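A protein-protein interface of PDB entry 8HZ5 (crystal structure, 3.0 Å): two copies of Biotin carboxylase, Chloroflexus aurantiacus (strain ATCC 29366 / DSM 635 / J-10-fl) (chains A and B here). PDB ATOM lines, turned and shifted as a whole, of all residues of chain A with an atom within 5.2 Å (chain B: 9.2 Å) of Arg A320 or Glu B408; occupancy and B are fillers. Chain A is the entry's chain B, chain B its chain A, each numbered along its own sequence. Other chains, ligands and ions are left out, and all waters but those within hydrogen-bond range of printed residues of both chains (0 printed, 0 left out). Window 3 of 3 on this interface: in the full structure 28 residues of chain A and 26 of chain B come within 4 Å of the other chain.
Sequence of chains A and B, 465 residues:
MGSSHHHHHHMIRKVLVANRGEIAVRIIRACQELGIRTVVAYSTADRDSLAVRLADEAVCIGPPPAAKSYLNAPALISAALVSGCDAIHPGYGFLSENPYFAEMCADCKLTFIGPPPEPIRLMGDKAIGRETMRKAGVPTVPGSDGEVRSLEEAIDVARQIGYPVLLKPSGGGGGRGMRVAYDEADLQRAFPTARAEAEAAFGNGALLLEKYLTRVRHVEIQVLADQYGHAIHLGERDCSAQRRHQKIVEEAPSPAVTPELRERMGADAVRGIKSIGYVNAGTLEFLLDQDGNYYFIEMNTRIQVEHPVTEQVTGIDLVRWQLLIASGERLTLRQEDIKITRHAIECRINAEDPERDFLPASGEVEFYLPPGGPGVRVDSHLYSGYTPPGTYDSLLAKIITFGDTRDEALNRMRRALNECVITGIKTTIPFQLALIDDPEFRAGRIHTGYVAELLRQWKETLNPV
No position is printed for both chains. Of the 8 pairs that touch across the chains among the printed residues, none has its exchanged pair printed and touching as well.
OE2 of Glu B408 lies within salt-bridge range of NH1 of Arg A320 (3.1 Å). The guanidinium group (NE) of Arg B412 lies within salt-bridge range of the side-chain carboxylate (OE2) of Glu A33. NH2 of Arg B412 lies within salt-bridge range of OD2 of Asp A317, at 3.0 Å. The side-chain carboxylate (OE2) of Glu A33 lies within salt-bridge range of the guanidinium group (NE) of Arg B415, 2.9 Å away. NH1 of Arg A320 sits close to NH2 of Arg B412, 3.3 Å away.
Printed residues of chain B within 4 Å of Arg A26: Pro B374. Printed residues of chain B within 4 Å of Glu A33: Pro B374 (3.9 Å), Arg B412 (3.2 Å) and Arg B415 (2.9 Å). Of the printed residues of chain B, Asp A317 touches Pro B374 (3.5 Å) and Arg B412 (3.0 Å). No residue of chain B comes within 4 Å of Val A319. Arg A320 touches just these residues of chain B: Glu B408 and Arg B412. Leu A323 touches none of the printed residues of chain B. His B343 touches none of the printed residues of chain A. Glu B408 touches one residue of chain A. Of the printed residues of chain A, Arg B415 touches Glu A33. The nearest printed residue of chain A that does not touch Glu B408 is Glu A33 (5.8 Å).
Among the printed residues, merely in contact across the chains: Asp A317 with Pro B374, Arg A26 with Pro B374 and Glu A33 with Pro B374.
Hydrophobic or aromatic side chains of chain B that line the printed part of chain A: Pro B374. Of the 12 printed residues of chain A, 4 touch a printed residue of chain B. Printed residues of chain A that touch a printed residue of chain B: Arg A26, Glu A33, Asp A317 and Arg A320. Among the printed residues, 8 pairs touch across the chains. Among the printed residues, Asp or Glu carboxylates within 4 Å of a Lys or Arg side-chain nitrogen of the other chain: Glu A33 with Arg B412, Glu A33 with Arg B415, Asp A317 with Arg B412 and Arg A320 with Glu B408.
NH2 of Arg B415 lies within hydrogen-bond range of O of Pro B374. OE1 of Glu B408 lies within hydrogen-bond range of N of Asp B404, at 3.0 Å. OE2 of Glu B408 lies within salt-bridge range of NH1 of Arg B412, at 3.5 Å. The side-chain carboxylate (OD1) of Asp A317 lies within salt-bridge range of the guanidinium group (NH2) of Arg A26 (2.7 Å). OD1 of Asp A317 lies within hydrogen-bond range of N of Val A319. N of Arg A320 is in hydrogen-bond range of OD1 of Asp A317 (3.0 Å).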
ATOM      1  N   ARG A  26      23.183 -27.865  25.521  1.00  0.00           N
ATOM      2  CA  ARG A  26      24.146 -27.387  24.539  1.00  0.00           C
ATOM      3  C   ARG A  26      24.701 -28.486  23.693  1.00  0.00           C
ATOM      4  O   ARG A  26      24.759 -28.358  22.490  1.00  0.00           O
ATOM      5  CB  ARG A  26      25.295 -26.728  25.281  1.00  0.00           C
ATOM      6  CG  ARG A  26      26.418 -26.185  24.439  1.00  0.00           C
ATOM      7  CD  ARG A  26      26.137 -24.758  24.046  1.00  0.00           C
ATOM      8  NE  ARG A  26      26.938 -24.387  22.900  1.00  0.00           N
ATOM      9  CZ  ARG A  26      26.868 -24.987  21.729  1.00  0.00           C
ATOM     10  NH1 ARG A  26      26.030 -25.987  21.534  1.00  0.00           N
ATOM     11  NH2 ARG A  26      27.641 -24.583  20.751  1.00  0.00           N
ATOM     12  N   ALA A  30      23.998 -29.352  19.754  1.00  0.00           N
ATOM     13  CA  ALA A  30      25.061 -29.464  18.808  1.00  0.00           C
ATOM     14  C   ALA A  30      25.040 -30.761  18.114  1.00  0.00           C
ATOM     15  O   ALA A  30      25.299 -30.846  16.934  1.00  0.00           O
ATOM     16  CB  ALA A  30      26.342 -29.326  19.541  1.00  0.00           C
ATOM     17  N   GLU A  33      22.313 -30.813  15.446  1.00  0.00           N
ATOM     18  CA  GLU A  33      22.701 -30.077  14.258  1.00  0.00           C
ATOM     19  C   GLU A  33      23.638 -30.872  13.381  1.00  0.00           C
ATOM     20  O   GLU A  33      23.698 -30.649  12.188  1.00  0.00           O
ATOM     21  CB  GLU A  33      23.346 -28.766  14.658  1.00  0.00           C
ATOM     22  CG  GLU A  33      22.412 -27.716  15.219  1.00  0.00           C
ATOM     23  CD  GLU A  33      23.167 -26.626  15.942  1.00  0.00           C
ATOM     24  OE1 GLU A  33      24.403 -26.621  15.886  1.00  0.00           O
ATOM     25  OE2 GLU A  33      22.532 -25.777  16.573  1.00  0.00           O
ATOM     26  N   LEU A  34      24.422 -31.750  13.977  1.00  0.00           N
ATOM     27  CA  LEU A  34      25.346 -32.593  13.240  1.00  0.00           C
ATOM     28  C   LEU A  34      24.798 -33.976  12.934  1.00  0.00           C
ATOM     29  O   LEU A  34      25.491 -34.786  12.354  1.00  0.00           O
ATOM     30  CB  LEU A  34      26.662 -32.681  13.986  1.00  0.00           C
ATOM     31  CG  LEU A  34      27.485 -31.420  14.159  1.00  0.00           C
ATOM     32  CD1 LEU A  34      28.645 -31.735  15.072  1.00  0.00           C
ATOM     33  CD2 LEU A  34      27.976 -30.912  12.819  1.00  0.00           C
ATOM     34  N   ASP A 317      31.317 -22.680  16.179  1.00  0.00           N
ATOM     35  CA  ASP A 317      30.665 -23.489  17.203  1.00  0.00           C
ATOM     36  C   ASP A 317      31.688 -24.385  17.836  1.00  0.00           C
ATOM     37  O   ASP A 317      32.218 -25.271  17.201  1.00  0.00           O
ATOM     38  CB  ASP A 317      29.560 -24.304  16.584  1.00  0.00           C
ATOM     39  CG  ASP A 317      28.504 -24.693  17.556  1.00  0.00           C
ATOM     40  OD1 ASP A 317      28.788 -25.507  18.440  1.00  0.00           O
ATOM     41  OD2 ASP A 317      27.369 -24.230  17.404  1.00  0.00           O
ATOM     42  N   LEU A 318      31.942 -24.175  19.108  1.00  0.00           N
ATOM     43  CA  LEU A 318      32.972 -24.905  19.775  1.00  0.00           C
ATOM     44  C   LEU A 318      32.567 -26.302  20.152  1.00  0.00           C
ATOM     45  O   LEU A 318      33.376 -27.203  20.112  1.00  0.00           O
ATOM     46  CB  LEU A 318      33.425 -24.106  20.988  1.00  0.00           C
ATOM     47  CG  LEU A 318      34.245 -22.861  20.702  1.00  0.00           C
ATOM     48  CD1 LEU A 318      34.309 -21.982  21.930  1.00  0.00           C
ATOM     49  CD2 LEU A 318      35.632 -23.269  20.258  1.00  0.00           C
ATOM     50  N   VAL A 319      31.305 -26.506  20.473  1.00  0.00           N
ATOM     51  CA  VAL A 319      30.864 -27.817  20.858  1.00  0.00           C
ATOM     52  C   VAL A 319      30.719 -28.699  19.649  1.00  0.00           C
ATOM     53  O   VAL A 319      31.066 -29.862  19.688  1.00  0.00           O
ATOM     54  CB  VAL A 319      29.650 -27.768  21.791  1.00  0.00           C
ATOM     55  CG1 VAL A 319      29.167 -29.160  22.157  1.00  0.00           C
ATOM     56  CG2 VAL A 319      30.014 -27.027  23.060  1.00  0.00           C
ATOM     57  N   ARG A 320      30.289 -28.148  18.538  1.00  0.00           N
ATOM     58  CA  ARG A 320      30.227 -28.923  17.317  1.00  0.00           C
ATOM     59  C   ARG A 320      31.586 -29.404  16.877  1.00  0.00           C
ATOM     60  O   ARG A 320      31.731 -30.507  16.416  1.00  0.00           O
ATOM     61  CB  ARG A 320      29.630 -28.103  16.195  1.00  0.00           C
ATOM     62  CG  ARG A 320      28.151 -28.283  15.911  1.00  0.00           C
ATOM     63  CD  ARG A 320      27.668 -27.081  15.119  1.00  0.00           C
ATOM     64  NE  ARG A 320      26.792 -27.371  14.001  1.00  0.00           N
ATOM     65  CZ  ARG A 320      26.603 -26.528  12.995  1.00  0.00           C
ATOM     66  NH1 ARG A 320      27.237 -25.371  12.983  1.00  0.00           N
ATOM     67  NH2 ARG A 320      25.787 -26.842  12.000  1.00  0.00           N
ATOM     68  N   TRP A 321      32.589 -28.576  17.037  1.00  0.00           N
ATOM     69  CA  TRP A 321      33.907 -28.941  16.616  1.00  0.00           C
ATOM     70  C   TRP A 321      34.497 -29.976  17.499  1.00  0.00           C
ATOM     71  O   TRP A 321      35.247 -30.793  17.047  1.00  0.00           O
ATOM     72  CB  TRP A 321      34.800 -27.734  16.534  1.00  0.00           C
ATOM     73  CG  TRP A 321      34.947 -27.236  15.151  1.00  0.00           C
ATOM     74  CD1 TRP A 321      34.472 -26.072  14.657  1.00  0.00           C
ATOM     75  CD2 TRP A 321      35.597 -27.899  14.064  1.00  0.00           C
ATOM     76  NE1 TRP A 321      34.786 -25.954  13.334  1.00  0.00           N
ATOM     77  CE2 TRP A 321      35.482 -27.066  12.945  1.00  0.00           C
ATOM     78  CE3 TRP A 321      36.268 -29.116  13.929  1.00  0.00           C
ATOM     79  CZ2 TRP A 321      36.010 -27.407  11.711  1.00  0.00           C
ATOM     80  CZ3 TRP A 321      36.785 -29.449  12.708  1.00  0.00           C
ATOM     81  CH2 TRP A 321      36.653 -28.600  11.613  1.00  0.00           C
ATOM     82  N   GLN A 322      34.145 -29.977  18.766  1.00  0.00           N
ATOM     83  CA  GLN A 322      34.600 -30.993  19.676  1.00  0.00           C
ATOM     84  C   GLN A 322      34.181 -32.341  19.205  1.00  0.00           C
ATOM     85  O   GLN A 322      34.980 -33.245  19.061  1.00  0.00           O
ATOM     86  CB  GLN A 322      33.930 -30.750  21.006  1.00  0.00           C
ATOM     87  CG  GLN A 322      34.620 -29.773  21.922  1.00  0.00           C
ATOM     88  CD  GLN A 322      33.955 -29.709  23.270  1.00  0.00           C
ATOM     89  OE1 GLN A 322      32.743 -29.764  23.376  1.00  0.00           O
ATOM     90  NE2 GLN A 322      34.749 -29.607  24.306  1.00  0.00           N
ATOM     91  N   LEU A 323      32.901 -32.493  18.978  1.00  0.00           N
ATOM     92  CA  LEU A 323      32.381 -33.748  18.497  1.00  0.00           C
ATOM     93  C   LEU A 323      32.968 -34.165  17.199  1.00  0.00           C
ATOM     94  O   LEU A 323      33.136 -35.335  16.960  1.00  0.00           O
ATOM     95  CB  LEU A 323      30.875 -33.636  18.352  1.00  0.00           C
ATOM     96  CG  LEU A 323      30.040 -33.112  19.512  1.00  0.00           C
ATOM     97  CD1 LEU A 323      28.822 -32.401  18.963  1.00  0.00           C
ATOM     98  CD2 LEU A 323      29.619 -34.262  20.401  1.00  0.00           C
ATOM     99  N   LEU A 324      33.318 -33.222  16.362  1.00  0.00           N
ATOM    100  CA  LEU A 324      33.947 -33.533  15.108  1.00  0.00           C
ATOM    101  C   LEU A 324      35.392 -33.969  15.225  1.00  0.00           C
ATOM    102  O   LEU A 324      35.792 -34.911  14.604  1.00  0.00           O
ATOM    103  CB  LEU A 324      33.808 -32.346  14.181  1.00  0.00           C
ATOM    104  CG  LEU A 324      32.440 -32.023  13.603  1.00  0.00           C
ATOM    105  CD1 LEU A 324      32.540 -30.791  12.721  1.00  0.00           C
ATOM    106  CD2 LEU A 324      31.854 -33.201  12.849  1.00  0.00           C
ATOM    107  N   THR B 341      27.253 -12.211   5.102  1.00  0.00           N
ATOM    108  CA  THR B 341      28.200 -13.129   5.687  1.00  0.00           C
ATOM    109  C   THR B 341      27.682 -14.485   6.066  1.00  0.00           C
ATOM    110  O   THR B 341      28.449 -15.432   6.167  1.00  0.00           O
ATOM    111  CB  THR B 341      28.740 -12.477   6.955  1.00  0.00           C
ATOM    112  OG1 THR B 341      27.646 -11.986   7.734  1.00  0.00           O
ATOM    113  CG2 THR B 341      29.644 -11.319   6.601  1.00  0.00           C
ATOM    114  N   ARG B 342      26.388 -14.617   6.241  1.00  0.00           N
ATOM    115  CA  ARG B 342      25.832 -15.856   6.728  1.00  0.00           C
ATOM    116  C   ARG B 342      24.609 -16.210   5.959  1.00  0.00           C
ATOM    117  O   ARG B 342      24.131 -15.401   5.192  1.00  0.00           O
ATOM    118  CB  ARG B 342      25.468 -15.722   8.214  1.00  0.00           C
ATOM    119  CG  ARG B 342      26.506 -15.036   9.072  1.00  0.00           C
ATOM    120  CD  ARG B 342      26.325 -15.326  10.542  1.00  0.00           C
ATOM    121  NE  ARG B 342      27.319 -14.615  11.334  1.00  0.00           N
ATOM    122  CZ  ARG B 342      28.530 -15.080  11.611  1.00  0.00           C
ATOM    123  NH1 ARG B 342      28.912 -16.265  11.159  1.00  0.00           N
ATOM    124  NH2 ARG B 342      29.367 -14.359  12.340  1.00  0.00           N
ATOM    125  N   HIS B 343      24.128 -17.437   6.103  1.00  0.00           N
ATOM    126  CA  HIS B 343      22.874 -17.785   5.497  1.00  0.00           C
ATOM    127  C   HIS B 343      21.802 -17.899   6.538  1.00  0.00           C
ATOM    128  O   HIS B 343      21.951 -18.632   7.473  1.00  0.00           O
ATOM    129  CB  HIS B 343      22.947 -19.037   4.675  1.00  0.00           C
ATOM    130  CG  HIS B 343      21.844 -19.156   3.671  1.00  0.00           C
ATOM    131  ND1 HIS B 343      20.523 -19.294   4.029  1.00  0.00           N
ATOM    132  CD2 HIS B 343      21.867 -19.146   2.316  1.00  0.00           C
ATOM    133  CE1 HIS B 343      19.777 -19.361   2.944  1.00  0.00           C
ATOM    134  NE2 HIS B 343      20.567 -19.272   1.891  1.00  0.00           N
ATOM    135  N   ALA B 344      20.705 -17.179   6.359  1.00  0.00           N
ATOM    136  CA  ALA B 344      19.636 -17.148   7.327  1.00  0.00           C
ATOM    137  C   ALA B 344      18.279 -17.476   6.786  1.00  0.00           C
ATOM    138  O   ALA B 344      17.966 -17.140   5.683  1.00  0.00           O
ATOM    139  CB  ALA B 344      19.595 -15.782   7.926  1.00  0.00           C
ATOM    140  N   ILE B 345      17.477 -18.169   7.564  1.00  0.00           N
ATOM    141  CA  ILE B 345      16.120 -18.479   7.179  1.00  0.00           C
ATOM    142  C   ILE B 345      15.164 -18.129   8.298  1.00  0.00           C
ATOM    143  O   ILE B 345      15.467 -18.355   9.444  1.00  0.00           O
ATOM    144  CB  ILE B 345      15.964 -19.961   6.782  1.00  0.00           C
ATOM    145  CG1 ILE B 345      14.505 -20.298   6.497  1.00  0.00           C
ATOM    146  CG2 ILE B 345      16.531 -20.885   7.843  1.00  0.00           C
ATOM    147  CD1 ILE B 345      14.248 -21.762   6.273  1.00  0.00           C
ATOM    148  N   PRO B 374      22.948 -21.803  20.122  1.00  0.00           N
ATOM    149  CA  PRO B 374      23.652 -21.315  18.957  1.00  0.00           C
ATOM    150  C   PRO B 374      22.806 -21.114  17.715  1.00  0.00           C
ATOM    151  O   PRO B 374      22.079 -22.000  17.325  1.00  0.00           O
ATOM    152  CB  PRO B 374      24.688 -22.400  18.732  1.00  0.00           C
ATOM    153  CG  PRO B 374      24.135 -23.624  19.354  1.00  0.00           C
ATOM    154  CD  PRO B 374      23.418 -23.126  20.557  1.00  0.00           C
ATOM    155  N   GLY B 375      22.885 -19.952  17.093  1.00  0.00           N
ATOM    156  CA  GLY B 375      22.199 -19.728  15.827  1.00  0.00           C
ATOM    157  C   GLY B 375      20.734 -19.494  15.762  1.00  0.00           C
ATOM    158  O   GLY B 375      20.152 -19.736  14.736  1.00  0.00           O
ATOM    159  N   VAL B 376      20.132 -19.035  16.845  1.00  0.00           N
ATOM    160  CA  VAL B 376      18.695 -18.859  16.919  1.00  0.00           C
ATOM    161  C   VAL B 376      18.317 -17.477  17.390  1.00  0.00           C
ATOM    162  O   VAL B 376      18.953 -16.941  18.279  1.00  0.00           O
ATOM    163  CB  VAL B 376      18.044 -19.884  17.881  1.00  0.00           C
ATOM    164  CG1 VAL B 376      16.539 -19.921  17.729  1.00  0.00           C
ATOM    165  CG2 VAL B 376      18.597 -21.276  17.676  1.00  0.00           C
ATOM    166  N   THR B 401      16.834 -18.691  12.009  1.00  0.00           N
ATOM    167  CA  THR B 401      18.057 -19.410  12.178  1.00  0.00           C
ATOM    168  C   THR B 401      19.099 -19.081  11.151  1.00  0.00           C
ATOM    169  O   THR B 401      18.807 -18.985   9.989  1.00  0.00           O
ATOM    170  CB  THR B 401      17.824 -20.914  12.254  1.00  0.00           C
ATOM    171  OG1 THR B 401      17.121 -21.351  11.100  1.00  0.00           O
ATOM    172  CG2 THR B 401      17.042 -21.257  13.503  1.00  0.00           C
ATOM    173  N   PHE B 402      20.326 -18.915  11.602  1.00  0.00           N
ATOM    174  CA  PHE B 402      21.416 -18.621  10.722  1.00  0.00           C
ATOM    175  C   PHE B 402      22.480 -19.675  10.710  1.00  0.00           C
ATOM    176  O   PHE B 402      22.454 -20.600  11.483  1.00  0.00           O
ATOM    177  CB  PHE B 402      22.027 -17.240  10.973  1.00  0.00           C
ATOM    178  CG  PHE B 402      22.342 -16.921  12.399  1.00  0.00           C
ATOM    179  CD1 PHE B 402      21.367 -16.455  13.257  1.00  0.00           C
ATOM    180  CD2 PHE B 402      23.638 -16.996  12.855  1.00  0.00           C
ATOM    181  CE1 PHE B 402      21.669 -16.139  14.559  1.00  0.00           C
ATOM    182  CE2 PHE B 402      23.950 -16.675  14.150  1.00  0.00           C
ATOM    183  CZ  PHE B 402      22.966 -16.242  15.004  1.00  0.00           C
ATOM    184  N   GLY B 403      23.404 -19.542   9.788  1.00  0.00           N
ATOM    185  CA  GLY B 403      24.477 -20.487   9.667  1.00  0.00           C
ATOM    186  C   GLY B 403      25.429 -19.986   8.628  1.00  0.00           C
ATOM    187  O   GLY B 403      25.245 -18.927   8.121  1.00  0.00           O
ATOM    188  N   ASP B 404      26.446 -20.752   8.308  1.00  0.00           N
ATOM    189  CA  ASP B 404      27.450 -20.313   7.367  1.00  0.00           C
ATOM    190  C   ASP B 404      27.144 -20.948   6.058  1.00  0.00           C
ATOM    191  O   ASP B 404      27.699 -20.572   5.048  1.00  0.00           O
ATOM    192  CB  ASP B 404      28.839 -20.713   7.856  1.00  0.00           C
ATOM    193  CG  ASP B 404      29.315 -19.890   9.032  1.00  0.00           C
ATOM    194  OD1 ASP B 404      28.662 -18.897   9.384  1.00  0.00           O
ATOM    195  OD2 ASP B 404      30.355 -20.241   9.608  1.00  0.00           O
ATOM    196  N   THR B 405      26.240 -21.908   6.064  1.00  0.00           N
ATOM    197  CA  THR B 405      25.806 -22.559   4.852  1.00  0.00           C
ATOM    198  C   THR B 405      24.288 -22.531   4.930  1.00  0.00           C
ATOM    199  O   THR B 405      23.743 -22.214   5.965  1.00  0.00           O
ATOM    200  CB  THR B 405      26.344 -24.002   4.738  1.00  0.00           C
ATOM    201  OG1 THR B 405      27.654 -24.081   5.297  1.00  0.00           O
ATOM    202  CG2 THR B 405      26.429 -24.444   3.299  1.00  0.00           C
ATOM    203  N   ARG B 406      23.598 -22.855   3.844  1.00  0.00           N
ATOM    204  CA  ARG B 406      22.143 -22.864   3.813  1.00  0.00           C
ATOM    205  C   ARG B 406      21.620 -24.034   4.526  1.00  0.00           C
ATOM    206  O   ARG B 406      20.619 -23.957   5.204  1.00  0.00           O
ATOM    207  CB  ARG B 406      21.631 -22.915   2.385  1.00  0.00           C
ATOM    208  CG  ARG B 406      20.129 -22.711   2.286  1.00  0.00           C
ATOM    209  CD  ARG B 406      19.606 -22.758   0.871  1.00  0.00           C
ATOM    210  NE  ARG B 406      18.178 -22.484   0.832  1.00  0.00           N
ATOM    211  CZ  ARG B 406      17.249 -23.384   0.537  1.00  0.00           C
ATOM    212  NH1 ARG B 406      17.589 -24.625   0.252  1.00  0.00           N
ATOM    213  NH2 ARG B 406      15.980 -23.037   0.522  1.00  0.00           N
ATOM    214  N   ASP B 407      22.324 -25.135   4.403  1.00  0.00           N
ATOM    215  CA  ASP B 407      21.925 -26.336   5.082  1.00  0.00           C
ATOM    216  C   ASP B 407      22.226 -26.291   6.557  1.00  0.00           C
ATOM    217  O   ASP B 407      21.552 -26.929   7.323  1.00  0.00           O
ATOM    218  CB  ASP B 407      22.522 -27.541   4.389  1.00  0.00           C
ATOM    219  CG  ASP B 407      21.610 -28.103   3.327  1.00  0.00           C
ATOM    220  OD1 ASP B 407      21.069 -27.313   2.534  1.00  0.00           O
ATOM    221  OD2 ASP B 407      21.429 -29.332   3.284  1.00  0.00           O
ATOM    222  N   GLU B 408      23.201 -25.513   6.983  1.00  0.00           N
ATOM    223  CA  GLU B 408      23.452 -25.338   8.391  1.00  0.00           C
ATOM    224  C   GLU B 408      22.292 -24.657   9.018  1.00  0.00           C
ATOM    225  O   GLU B 408      21.832 -25.060  10.062  1.00  0.00           O
ATOM    226  CB  GLU B 408      24.673 -24.487   8.584  1.00  0.00           C
ATOM    227  CG  GLU B 408      25.002 -24.148  10.021  1.00  0.00           C
ATOM    228  CD  GLU B 408      26.341 -23.468  10.146  1.00  0.00           C
ATOM    229  OE1 GLU B 408      27.117 -23.525   9.183  1.00  0.00           O
ATOM    230  OE2 GLU B 408      26.609 -22.867  11.198  1.00  0.00           O
ATOM    231  N   ALA B 409      21.765 -23.648   8.364  1.00  0.00           N
ATOM    232  CA  ALA B 409      20.644 -22.907   8.862  1.00  0.00           C
ATOM    233  C   ALA B 409      19.377 -23.662   8.832  1.00  0.00           C
ATOM    234  O   ALA B 409      18.504 -23.425   9.633  1.00  0.00           O
ATOM    235  CB  ALA B 409      20.486 -21.703   7.992  1.00  0.00           C
ATOM    236  N   LEU B 410      19.249 -24.568   7.897  1.00  0.00           N
ATOM    237  CA  LEU B 410      18.033 -25.307   7.753  1.00  0.00           C
ATOM    238  C   LEU B 410      18.000 -26.380   8.777  1.00  0.00           C
ATOM    239  O   LEU B 410      16.943 -26.800   9.207  1.00  0.00           O
ATOM    240  CB  LEU B 410      17.993 -25.923   6.378  1.00  0.00           C
ATOM    241  CG  LEU B 410      17.374 -25.122   5.248  1.00  0.00           C
ATOM    242  CD1 LEU B 410      17.430 -25.933   3.968  1.00  0.00           C
ATOM    243  CD2 LEU B 410      15.942 -24.845   5.628  1.00  0.00           C
ATOM    244  N   ASN B 411      19.163 -26.831   9.186  1.00  0.00           N
ATOM    245  CA  ASN B 411      19.251 -27.850  10.192  1.00  0.00           C
ATOM    246  C   ASN B 411      19.144 -27.274  11.585  1.00  0.00           C
ATOM    247  O   ASN B 411      18.756 -27.965  12.512  1.00  0.00           O
ATOM    248  CB  ASN B 411      20.549 -28.633  10.013  1.00  0.00           C
ATOM    249  CG  ASN B 411      20.555 -29.485   8.767  1.00  0.00           C
ATOM    250  OD1 ASN B 411      19.513 -29.806   8.208  1.00  0.00           O
ATOM    251  ND2 ASN B 411      21.741 -29.847   8.316  1.00  0.00           N
ATOM    252  N   ARG B 412      19.471 -26.006  11.757  1.00  0.00           N
ATOM    253  CA  ARG B 412      19.309 -25.369  13.041  1.00  0.00           C
ATOM    254  C   ARG B 412      17.891 -24.983  13.292  1.00  0.00           C
ATOM    255  O   ARG B 412      17.497 -24.820  14.427  1.00  0.00           O
ATOM    256  CB  ARG B 412      20.193 -24.143  13.155  1.00  0.00           C
ATOM    257  CG  ARG B 412      21.667 -24.417  13.312  1.00  0.00           C
ATOM    258  CD  ARG B 412      22.375 -23.204  13.869  1.00  0.00           C
ATOM    259  NE  ARG B 412      23.648 -23.555  14.482  1.00  0.00           N
ATOM    260  CZ  ARG B 412      24.718 -22.780  14.459  1.00  0.00           C
ATOM    261  NH1 ARG B 412      24.674 -21.609  13.851  1.00  0.00           N
ATOM    262  NH2 ARG B 412      25.831 -23.174  15.039  1.00  0.00           N
ATOM    263  N   MET B 413      17.103 -24.858  12.240  1.00  0.00           N
ATOM    264  CA  MET B 413      15.699 -24.565  12.378  1.00  0.00           C
ATOM    265  C   MET B 413      14.988 -25.816  12.701  1.00  0.00           C
ATOM    266  O   MET B 413      14.009 -25.812  13.399  1.00  0.00           O
ATOM    267  CB  MET B 413      15.128 -24.109  11.052  1.00  0.00           C
ATOM    268  CG  MET B 413      13.710 -23.578  11.087  1.00  0.00           C
ATOM    269  SD  MET B 413      13.475 -22.095  12.069  1.00  0.00           S
ATOM    270  CE  MET B 413      13.954 -20.889  10.869  1.00  0.00           C
ATOM    271  N   ARG B 414      15.510 -26.910  12.203  1.00  0.00           N
ATOM    272  CA  ARG B 414      14.940 -28.189  12.461  1.00  0.00           C
ATOM    273  C   ARG B 414      14.919 -28.310  13.930  1.00  0.00           C
ATOM    274  O   ARG B 414      13.908 -28.633  14.508  1.00  0.00           O
ATOM    275  CB  ARG B 414      15.805 -29.284  11.888  1.00  0.00           C
ATOM    276  CG  ARG B 414      15.126 -30.239  10.942  1.00  0.00           C
ATOM    277  CD  ARG B 414      16.153 -30.800   9.987  1.00  0.00           C
ATOM    278  NE  ARG B 414      16.891 -31.917  10.560  1.00  0.00           N
ATOM    279  CZ  ARG B 414      17.975 -32.449  10.008  1.00  0.00           C
ATOM    280  NH1 ARG B 414      18.453 -31.960   8.877  1.00  0.00           N
ATOM    281  NH2 ARG B 414      18.590 -33.466  10.589  1.00  0.00           N
ATOM    282  N   ARG B 415      16.042 -28.044  14.555  1.00  0.00           N
ATOM    283  CA  ARG B 415      16.159 -28.193  15.982  1.00  0.00           C
ATOM    284  C   ARG B 415      15.299 -27.249  16.713  1.00  0.00           C
ATOM    285  O   ARG B 415      14.550 -27.649  17.568  1.00  0.00           O
ATOM    286  CB  ARG B 415      17.616 -27.961  16.356  1.00  0.00           C
ATOM    287  CG  ARG B 415      17.849 -27.698  17.811  1.00  0.00           C
ATOM    288  CD  ARG B 415      19.319 -27.646  18.089  1.00  0.00           C
ATOM    289  NE  ARG B 415      19.982 -26.399  17.706  1.00  0.00           N
ATOM    290  CZ  ARG B 415      19.831 -25.227  18.310  1.00  0.00           C
ATOM    291  NH1 ARG B 415      18.998 -25.069  19.319  1.00  0.00           N
ATOM    292  NH2 ARG B 415      20.515 -24.195  17.877  1.00  0.00           N
ATOM    293  N   ALA B 416      15.354 -25.992  16.343  1.00  0.00           N
ATOM    294  CA  ALA B 416      14.588 -24.968  17.003  1.00  0.00           C
ATOM    295  C   ALA B 416      13.098 -25.009  16.844  1.00  0.00           C
ATOM    296  O   ALA B 416      12.385 -24.315  17.531  1.00  0.00           O
ATOM    297  CB  ALA B 416      15.081 -23.664  16.515  1.00  0.00           C
